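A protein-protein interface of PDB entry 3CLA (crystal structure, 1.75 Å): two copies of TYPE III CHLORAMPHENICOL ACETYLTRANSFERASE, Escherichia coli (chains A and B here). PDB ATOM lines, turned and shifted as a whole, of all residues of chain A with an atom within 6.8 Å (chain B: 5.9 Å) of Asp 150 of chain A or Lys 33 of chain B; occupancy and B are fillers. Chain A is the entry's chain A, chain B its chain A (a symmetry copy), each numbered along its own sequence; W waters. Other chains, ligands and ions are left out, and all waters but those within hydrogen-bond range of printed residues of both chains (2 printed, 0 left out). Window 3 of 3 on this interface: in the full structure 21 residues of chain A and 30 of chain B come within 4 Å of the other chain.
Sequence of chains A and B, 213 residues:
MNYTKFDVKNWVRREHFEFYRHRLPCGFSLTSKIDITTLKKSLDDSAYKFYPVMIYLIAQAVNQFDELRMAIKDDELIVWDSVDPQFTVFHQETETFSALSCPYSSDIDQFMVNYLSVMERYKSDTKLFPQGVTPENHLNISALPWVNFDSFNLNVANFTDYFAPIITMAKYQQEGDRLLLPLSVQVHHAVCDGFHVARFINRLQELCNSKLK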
ATOM      1  N   LEU A  30      30.211  15.243 -17.525  1.00  0.00           N
ATOM      2  CA  LEU A  30      29.197  15.413 -16.473  1.00  0.00           C
ATOM      3  C   LEU A  30      27.940  14.617 -16.911  1.00  0.00           C
ATOM      4  O   LEU A  30      27.675  14.633 -18.121  1.00  0.00           O
ATOM      5  CB  LEU A  30      28.965  16.874 -16.144  1.00  0.00           C
ATOM      6  CG  LEU A  30      28.137  17.865 -16.800  1.00  0.00           C
ATOM      7  CD1 LEU A  30      26.619  17.635 -16.569  1.00  0.00           C
ATOM      8  CD2 LEU A  30      28.353  19.209 -16.090  1.00  0.00           C
ATOM      9  N   THR A  31      27.263  14.023 -15.932  1.00  0.00           N
ATOM     10  CA  THR A  31      26.010  13.334 -16.312  1.00  0.00           C
ATOM     11  C   THR A  31      24.927  14.038 -15.469  1.00  0.00           C
ATOM     12  O   THR A  31      25.141  14.265 -14.245  1.00  0.00           O
ATOM     13  CB  THR A  31      26.017  11.808 -15.954  1.00  0.00           C
ATOM     14  OG1 THR A  31      27.322  11.374 -16.444  1.00  0.00           O
ATOM     15  CG2 THR A  31      24.781  11.036 -16.436  1.00  0.00           C
ATOM     16  N   SER A  32      23.852  14.317 -16.193  1.00  0.00           N
ATOM     17  CA  SER A  32      22.750  15.031 -15.455  1.00  0.00           C
ATOM     18  C   SER A  32      21.476  14.309 -15.916  1.00  0.00           C
ATOM     19  O   SER A  32      21.467  13.643 -16.962  1.00  0.00           O
ATOM     20  CB  SER A  32      22.867  16.492 -15.982  1.00  0.00           C
ATOM     21  OG  SER A  32      21.827  17.235 -15.369  1.00  0.00           O
ATOM     22  N   LYS A  33      20.387  14.442 -15.206  1.00  0.00           N
ATOM     23  CA  LYS A  33      19.143  13.789 -15.675  1.00  0.00           C
ATOM     24  C   LYS A  33      18.221  14.863 -16.274  1.00  0.00           C
ATOM     25  O   LYS A  33      18.017  15.898 -15.652  1.00  0.00           O
ATOM     26  CB  LYS A  33      18.505  13.137 -14.462  1.00  0.00           C
ATOM     27  CG  LYS A  33      19.353  11.871 -14.056  1.00  0.00           C
ATOM     28  CD  LYS A  33      18.664  11.213 -12.895  1.00  0.00           C
ATOM     29  CE  LYS A  33      19.174   9.768 -12.782  1.00  0.00           C
ATOM     30  NZ  LYS A  33      20.623   9.843 -12.518  1.00  0.00           N
ATOM     31  N   ASN A 148      20.247   1.620 -17.043  1.00  0.00           N
ATOM     32  CA  ASN A 148      20.211   3.001 -16.545  1.00  0.00           C
ATOM     33  C   ASN A 148      21.605   3.232 -15.912  1.00  0.00           C
ATOM     34  O   ASN A 148      22.196   2.266 -15.356  1.00  0.00           O
ATOM     35  CB  ASN A 148      19.097   3.090 -15.483  1.00  0.00           C
ATOM     36  CG  ASN A 148      18.945   4.469 -14.869  1.00  0.00           C
ATOM     37  OD1 ASN A 148      19.515   4.631 -13.763  1.00  0.00           O
ATOM     38  ND2 ASN A 148      18.317   5.401 -15.573  1.00  0.00           N
ATOM     39  N   PHE A 149      22.091   4.447 -15.962  1.00  0.00           N
ATOM     40  CA  PHE A 149      23.384   4.759 -15.303  1.00  0.00           C
ATOM     41  C   PHE A 149      23.187   6.127 -14.667  1.00  0.00           C
ATOM     42  O   PHE A 149      22.379   6.929 -15.160  1.00  0.00           O
ATOM     43  CB  PHE A 149      24.624   4.687 -16.222  1.00  0.00           C
ATOM     44  CG  PHE A 149      24.689   5.577 -17.435  1.00  0.00           C
ATOM     45  CD1 PHE A 149      24.686   6.965 -17.354  1.00  0.00           C
ATOM     46  CD2 PHE A 149      24.804   4.964 -18.717  1.00  0.00           C
ATOM     47  CE1 PHE A 149      24.755   7.763 -18.516  1.00  0.00           C
ATOM     48  CE2 PHE A 149      24.937   5.766 -19.842  1.00  0.00           C
ATOM     49  CZ  PHE A 149      24.878   7.181 -19.779  1.00  0.00           C
ATOM     50  N   ASP A 150      23.998   6.413 -13.695  1.00  0.00           N
ATOM     51  CA  ASP A 150      24.040   7.747 -13.064  1.00  0.00           C
ATOM     52  C   ASP A 150      25.308   8.487 -13.576  1.00  0.00           C
ATOM     53  O   ASP A 150      25.331   9.709 -13.381  1.00  0.00           O
ATOM     54  CB  ASP A 150      24.091   7.642 -11.528  1.00  0.00           C
ATOM     55  CG  ASP A 150      22.803   6.913 -11.089  1.00  0.00           C
ATOM     56  OD1 ASP A 150      21.781   7.568 -11.307  1.00  0.00           O
ATOM     57  OD2 ASP A 150      22.849   5.745 -10.712  1.00  0.00           O
ATOM     58  N   SER A 151      26.243   7.713 -14.132  1.00  0.00           N
ATOM     59  CA  SER A 151      27.438   8.353 -14.648  1.00  0.00           C
ATOM     60  C   SER A 151      27.990   7.579 -15.811  1.00  0.00           C
ATOM     61  O   SER A 151      27.841   6.344 -15.864  1.00  0.00           O
ATOM     62  CB  SER A 151      28.558   8.498 -13.567  1.00  0.00           C
ATOM     63  OG  SER A 151      29.377   7.400 -13.536  1.00  0.00           O
ATOM     64  N   PHE A 152      28.697   8.326 -16.680  1.00  0.00           N
ATOM     65  CA  PHE A 152      29.353   7.635 -17.788  1.00  0.00           C
ATOM     66  C   PHE A 152      30.607   8.502 -18.112  1.00  0.00           C
ATOM     67  O   PHE A 152      30.411   9.754 -18.205  1.00  0.00           O
ATOM     68  CB  PHE A 152      28.375   7.617 -19.048  1.00  0.00           C
ATOM     69  CG  PHE A 152      29.005   6.877 -20.215  1.00  0.00           C
ATOM     70  CD1 PHE A 152      28.915   5.455 -20.320  1.00  0.00           C
ATOM     71  CD2 PHE A 152      29.717   7.607 -21.190  1.00  0.00           C
ATOM     72  CE1 PHE A 152      29.518   4.756 -21.374  1.00  0.00           C
ATOM     73  CE2 PHE A 152      30.357   6.925 -22.237  1.00  0.00           C
ATOM     74  CZ  PHE A 152      30.269   5.510 -22.309  1.00  0.00           C
ATOM     75  N   ALA A 170      21.368   7.059 -21.419  1.00  0.00           N
ATOM     76  CA  ALA A 170      21.116   5.712 -20.833  1.00  0.00           C
ATOM     77  C   ALA A 170      19.632   5.357 -20.945  1.00  0.00           C
ATOM     78  O   ALA A 170      18.863   6.178 -21.463  1.00  0.00           O
ATOM     79  CB  ALA A 170      21.473   5.779 -19.343  1.00  0.00           C
ATOM     80  N   GLN A 173      14.197   6.279 -16.704  1.00  0.00           N
ATOM     81  CA  GLN A 173      13.468   5.510 -15.640  1.00  0.00           C
ATOM     82  C   GLN A 173      12.554   6.496 -14.906  1.00  0.00           C
ATOM     83  O   GLN A 173      12.817   7.671 -14.902  1.00  0.00           O
ATOM     84  CB  GLN A 173      14.334   4.675 -14.797  1.00  0.00           C
ATOM     85  CG  GLN A 173      15.052   5.260 -13.624  1.00  0.00           C
ATOM     86  CD  GLN A 173      15.785   4.171 -12.837  1.00  0.00           C
ATOM     87  OE1 GLN A 173      16.066   4.330 -11.648  1.00  0.00           O
ATOM     88  NE2 GLN A 173      16.073   3.037 -13.466  1.00  0.00           N
ATOM     89  N   PRO A 182      19.089   9.896 -18.057  1.00  0.00           N
ATOM     90  CA  PRO A 182      20.513  10.213 -17.787  1.00  0.00           C
ATOM     91  C   PRO A 182      21.186  10.561 -19.144  1.00  0.00           C
ATOM     92  O   PRO A 182      21.079   9.822 -20.146  1.00  0.00           O
ATOM     93  CB  PRO A 182      21.110   8.949 -17.196  1.00  0.00           C
ATOM     94  CG  PRO A 182      19.901   8.063 -16.802  1.00  0.00           C
ATOM     95  CD  PRO A 182      18.854   8.466 -17.886  1.00  0.00           C
ATOM     96  N   THR B  31      28.451   4.034 -13.780  1.00  0.00           N
ATOM     97  CA  THR B  31      28.045   3.588 -12.428  1.00  0.00           C
ATOM     98  C   THR B  31      26.512   3.454 -12.525  1.00  0.00           C
ATOM     99  O   THR B  31      25.841   4.368 -13.084  1.00  0.00           O
ATOM    100  CB  THR B  31      28.392   4.628 -11.310  1.00  0.00           C
ATOM    101  OG1 THR B  31      29.771   4.988 -11.629  1.00  0.00           O
ATOM    102  CG2 THR B  31      28.091   4.153  -9.882  1.00  0.00           C
ATOM    103  N   SER B  32      26.085   2.330 -11.966  1.00  0.00           N
ATOM    104  CA  SER B  32      24.597   2.103 -12.037  1.00  0.00           C
ATOM    105  C   SER B  32      24.238   1.603 -10.632  1.00  0.00           C
ATOM    106  O   SER B  32      25.107   1.127  -9.885  1.00  0.00           O
ATOM    107  CB  SER B  32      24.464   1.013 -13.143  1.00  0.00           C
ATOM    108  OG  SER B  32      23.085   0.701 -13.247  1.00  0.00           O
ATOM    109  N   LYS B  33      22.990   1.650 -10.248  1.00  0.00           N
ATOM    110  CA  LYS B  33      22.631   1.120  -8.913  1.00  0.00           C
ATOM    111  C   LYS B  33      21.947  -0.244  -9.092  1.00  0.00           C
ATOM    112  O   LYS B  33      21.048  -0.364  -9.916  1.00  0.00           O
ATOM    113  CB  LYS B  33      21.685   2.126  -8.282  1.00  0.00           C
ATOM    114  CG  LYS B  33      22.504   3.408  -7.867  1.00  0.00           C
ATOM    115  CD  LYS B  33      21.556   4.356  -7.190  1.00  0.00           C
ATOM    116  CE  LYS B  33      22.378   5.368  -6.377  1.00  0.00           C
ATOM    117  NZ  LYS B  33      23.218   6.110  -7.336  1.00  0.00           N
ATOM    118  N   ILE B  34      22.503  -1.188  -8.353  1.00  0.00           N
ATOM    119  CA  ILE B  34      21.879  -2.550  -8.350  1.00  0.00           C
ATOM    120  C   ILE B  34      20.901  -2.603  -7.154  1.00  0.00           C
ATOM    121  O   ILE B  34      21.287  -2.178  -6.044  1.00  0.00           O
ATOM    122  CB  ILE B  34      23.045  -3.567  -8.169  1.00  0.00           C
ATOM    123  CG1 ILE B  34      24.044  -3.503  -9.404  1.00  0.00           C
ATOM    124  CG2 ILE B  34      22.643  -5.036  -7.898  1.00  0.00           C
ATOM    125  CD1 ILE B  34      23.248  -3.719 -10.738  1.00  0.00           C
ATOM    126  N   ASP B  35      19.739  -3.142  -7.427  1.00  0.00           N
ATOM    127  CA  ASP B  35      18.761  -3.356  -6.297  1.00  0.00           C
ATOM    128  C   ASP B  35      19.161  -4.641  -5.504  1.00  0.00           C
ATOM    129  O   ASP B  35      19.075  -5.771  -5.996  1.00  0.00           O
ATOM    130  CB  ASP B  35      17.385  -3.442  -6.927  1.00  0.00           C
ATOM    131  CG  ASP B  35      16.260  -3.640  -5.913  1.00  0.00           C
ATOM    132  OD1 ASP B  35      15.091  -3.640  -6.365  1.00  0.00           O
ATOM    133  OD2 ASP B  35      16.570  -3.748  -4.721  1.00  0.00           O
ATOM    134  N   ASN B 148      28.694   6.588   0.281  1.00  0.00           N
ATOM    135  CA  ASN B 148      27.863   6.266  -0.886  1.00  0.00           C
ATOM    136  C   ASN B 148      28.382   7.193  -2.013  1.00  0.00           C
ATOM    137  O   ASN B 148      28.819   8.339  -1.714  1.00  0.00           O
ATOM    138  CB  ASN B 148      26.399   6.597  -0.526  1.00  0.00           C
ATOM    139  CG  ASN B 148      25.417   6.320  -1.649  1.00  0.00           C
ATOM    140  OD1 ASN B 148      25.092   7.316  -2.339  1.00  0.00           O
ATOM    141  ND2 ASN B 148      25.055   5.062  -1.867  1.00  0.00           N
ATOM    142  N   PHE B 149      28.312   6.741  -3.240  1.00  0.00           N
ATOM    143  CA  PHE B 149      28.715   7.606  -4.376  1.00  0.00           C
ATOM    144  C   PHE B 149      27.691   7.332  -5.468  1.00  0.00           C
ATOM    145  O   PHE B 149      27.123   6.231  -5.522  1.00  0.00           O
ATOM    146  CB  PHE B 149      30.174   7.427  -4.851  1.00  0.00           C
ATOM    147  CG  PHE B 149      30.628   6.076  -5.335  1.00  0.00           C
ATOM    148  CD1 PHE B 149      30.068   5.443  -6.440  1.00  0.00           C
ATOM    149  CD2 PHE B 149      31.707   5.442  -4.654  1.00  0.00           C
ATOM    150  CE1 PHE B 149      30.526   4.178  -6.864  1.00  0.00           C
ATOM    151  CE2 PHE B 149      32.187   4.227  -5.126  1.00  0.00           C
ATOM    152  CZ  PHE B 149      31.589   3.545  -6.216  1.00  0.00           C
ATOM    153  N   ASP B 150      27.574   8.261  -6.368  1.00  0.00           N
ATOM    154  CA  ASP B 150      26.735   8.097  -7.571  1.00  0.00           C
ATOM    155  C   ASP B 150      27.670   7.837  -8.785  1.00  0.00           C
ATOM    156  O   ASP B 150      27.122   7.386  -9.798  1.00  0.00           O
ATOM    157  CB  ASP B 150      25.882   9.351  -7.838  1.00  0.00           C
ATOM    158  CG  ASP B 150      24.971   9.541  -6.606  1.00  0.00           C
ATOM    159  OD1 ASP B 150      24.140   8.639  -6.479  1.00  0.00           O
ATOM    160  OD2 ASP B 150      25.204  10.433  -5.794  1.00  0.00           O
ATOM    161  N   SER B 151      28.952   8.168  -8.606  1.00  0.00           N
ATOM    162  CA  SER B 151      29.875   7.926  -9.699  1.00  0.00           C
ATOM    163  C   SER B 151      31.252   7.638  -9.171  1.00  0.00           C
ATOM    164  O   SER B 151      31.630   8.154  -8.104  1.00  0.00           O
ATOM    165  CB  SER B 151      29.963   9.130 -10.691  1.00  0.00           C
ATOM    166  OG  SER B 151      30.926  10.028 -10.313  1.00  0.00           O
ATOM    167  N   LEU B 180      19.655   0.157  -2.465  1.00  0.00           N
ATOM    168  CA  LEU B 180      20.467   0.229  -3.710  1.00  0.00           C
ATOM    169  C   LEU B 180      21.974   0.258  -3.486  1.00  0.00           C
ATOM    170  O   LEU B 180      22.475   0.999  -2.626  1.00  0.00           O
ATOM    171  CB  LEU B 180      20.009   1.502  -4.432  1.00  0.00           C
ATOM    172  CG  LEU B 180      18.530   1.563  -4.733  1.00  0.00           C
ATOM    173  CD1 LEU B 180      18.242   2.916  -5.432  1.00  0.00           C
ATOM    174  CD2 LEU B 180      18.122   0.427  -5.656  1.00  0.00           C
ATOM    175  N   LEU B 181      22.677  -0.496  -4.306  1.00  0.00           N
ATOM    176  CA  LEU B 181      24.158  -0.525  -4.206  1.00  0.00           C
ATOM    177  C   LEU B 181      24.749   0.122  -5.493  1.00  0.00           C
ATOM    178  O   LEU B 181      24.564  -0.467  -6.585  1.00  0.00           O
ATOM    179  CB  LEU B 181      24.546  -2.028  -4.110  1.00  0.00           C
ATOM    180  CG  LEU B 181      26.058  -2.269  -4.187  1.00  0.00           C
ATOM    181  CD1 LEU B 181      26.662  -2.019  -2.823  1.00  0.00           C
ATOM    182  CD2 LEU B 181      26.297  -3.693  -4.639  1.00  0.00           C
ATOM    183  N   PRO B 182      25.456   1.211  -5.328  1.00  0.00           N
ATOM    184  CA  PRO B 182      26.186   1.827  -6.464  1.00  0.00           C
ATOM    185  C   PRO B 182      27.354   0.876  -6.848  1.00  0.00           C
ATOM    186  O   PRO B 182      28.153   0.432  -5.996  1.00  0.00           O
ATOM    187  CB  PRO B 182      26.714   3.151  -5.943  1.00  0.00           C
ATOM    188  CG  PRO B 182      25.945   3.416  -4.625  1.00  0.00           C
ATOM    189  CD  PRO B 182      25.710   1.965  -4.105  1.00  0.00           C
ATOM    190  N   LEU B 183      27.439   0.603  -8.140  1.00  0.00           N
ATOM    191  CA  LEU B 183      28.491  -0.285  -8.702  1.00  0.00           C
ATOM    192  C   LEU B 183      29.006   0.396  -9.985  1.00  0.00           C
ATOM    193  O   LEU B 183      28.248   0.671 -10.914  1.00  0.00           O
ATOM    194  CB  LEU B 183      27.841  -1.632  -9.061  1.00  0.00           C
ATOM    195  CG  LEU B 183      28.825  -2.719  -9.503  1.00  0.00           C
ATOM    196  CD1 LEU B 183      28.883  -3.762  -8.400  1.00  0.00           C
ATOM    197  CD2 LEU B 183      28.260  -3.399 -10.746  1.00  0.00           C
ATOM    198  N   GLN B 205      22.249  -8.220 -11.626  1.00  0.00           N
ATOM    199  CA  GLN B 205      20.970  -7.912 -10.948  1.00  0.00           C
ATOM    200  C   GLN B 205      20.098  -9.186 -10.814  1.00  0.00           C
ATOM    201  O   GLN B 205      19.499  -9.471  -9.742  1.00  0.00           O
ATOM    202  CB  GLN B 205      20.259  -6.825 -11.748  1.00  0.00           C
ATOM    203  CG  GLN B 205      18.853  -6.530 -11.187  1.00  0.00           C
ATOM    204  CD  GLN B 205      18.984  -5.883  -9.819  1.00  0.00           C
ATOM    205  OE1 GLN B 205      19.244  -4.686  -9.749  1.00  0.00           O
ATOM    206  NE2 GLN B 205      18.848  -6.681  -8.771  1.00  0.00           N
HETATM  207  O   HOH W   1      21.459   3.722 -11.957  1.00  0.00           O
HETATM  208  O   HOH W   2      25.125   5.350  -9.202  1.00  0.00           O
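O of Thr 31 of chain B lies within hydrogen-bond range of N of Asp 150 of chain A (2.8 Å). The backbone carbonyl oxygen of Asn 148 of chain A sits at hydrogen-bond distance from the side-chain hydroxyl of Ser 32 of chain B, 2.8 Å away. The side-chain carboxylate (OD2) of Asp 150 of chain A is in salt-bridge range of the side-chain amino group (NZ) of Lys 33 of chain B (3.4 Å). OG of Ser 151 of chain A sits at hydrogen-bond distance from OG1 of Thr 31 of chain B (3.1 Å).
Water W1 lies within hydrogen-bond range of the side-chain carboxylate of Asp 150 of chain A (2.8 Å), the side-chain amide oxygen of Asn 148 of chain A (2.8 Å) and the backbone NH of Lys 33 of chain B (3.1 Å). Water W2 lies within hydrogen-bond range of OD2 of Asp 150 of chain A (2.8 Å), NZ of Lys 33 of chain B (2.8 Å) and O of Asp 150 of chain B (2.9 Å).
Phe 149 of chain A touches Thr 31 of chain B, but with the chains exchanged Thr 31 of chain A does not touch Phe 149 of chain B (11.5 Å). Asp 150 of chain A touches Thr 31 of chain B, but with the chains exchanged Thr 31 of chain A does not touch Asp 150 of chain B (7.7 Å). Asp 150 of chain A touches Lys 33 of chain B, but with the chains exchanged Lys 33 of chain A does not touch Asp 150 of chain B (7.1 Å). Ser 151 of chain A touches its own counterpart, Ser 151 of chain B.
Of the 14 printed residues of chain B, 5 touch a printed residue of chain A. Hydrophobic or aromatic side chains of chain A within 4 Å of the printed part of chain B: Phe 149. Among the printed residues, 7 pairs touch across the chains. Among the printed residues, Asp or Glu carboxylates within 4 Å of a Lys or Arg side-chain nitrogen of the other chain: Asp 150 of chain A with Lys 33 of chain B (3.4 Å).
Thr 31 of chain B touches Phe 149 of chain A (O to CA, 3.3 Å). Asp 150 of chain B touches Asp 150 of chain A (O to CB, 3.5 Å). CB of Ser 151 of chain A touches CB of Ser 151 of chain B (3.3 Å).
Asp 150 of chain A touches just these residues of chain B: Thr 31, Lys 33 and Asp 150. Lys 33 of chain B touches one residue of chain A. Of the printed residues of chain A, Thr 31 of chain B touches Phe 149, Asp 150 and Ser 151. Of the printed residues of chain A, Ser 151 of chain B touches Ser 151. Printed residues of chain A within 4 Å of Ser 32 of chain B: Asn 148 (2.8 Å). Printed residues of chain A within 4 Å of Asp 150 of chain B: Asp 150. Pro 182 of chain A touches none of the printed residues of chain B. The nearest residue of chain B that does not touch Asp 150 of chain A is Ser 32 of chain B (4.3 Å). The nearest printed residue of chain B that does not touch Phe 149 of chain A is Ser 32 of chain B (4.4 Å).
The side-chain amino group of Lys 33 of chain B is in salt-bridge range of the side-chain carboxylate of Asp 150 of chain B, at 2.8 Å. N of Ser 32 of chain B lies within hydrogen-bond range of O of Leu 183 of chain B (2.9 Å). NZ of Lys 33 of chain A lies within salt-bridge range of OD1 of Asp 150 of chain A.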
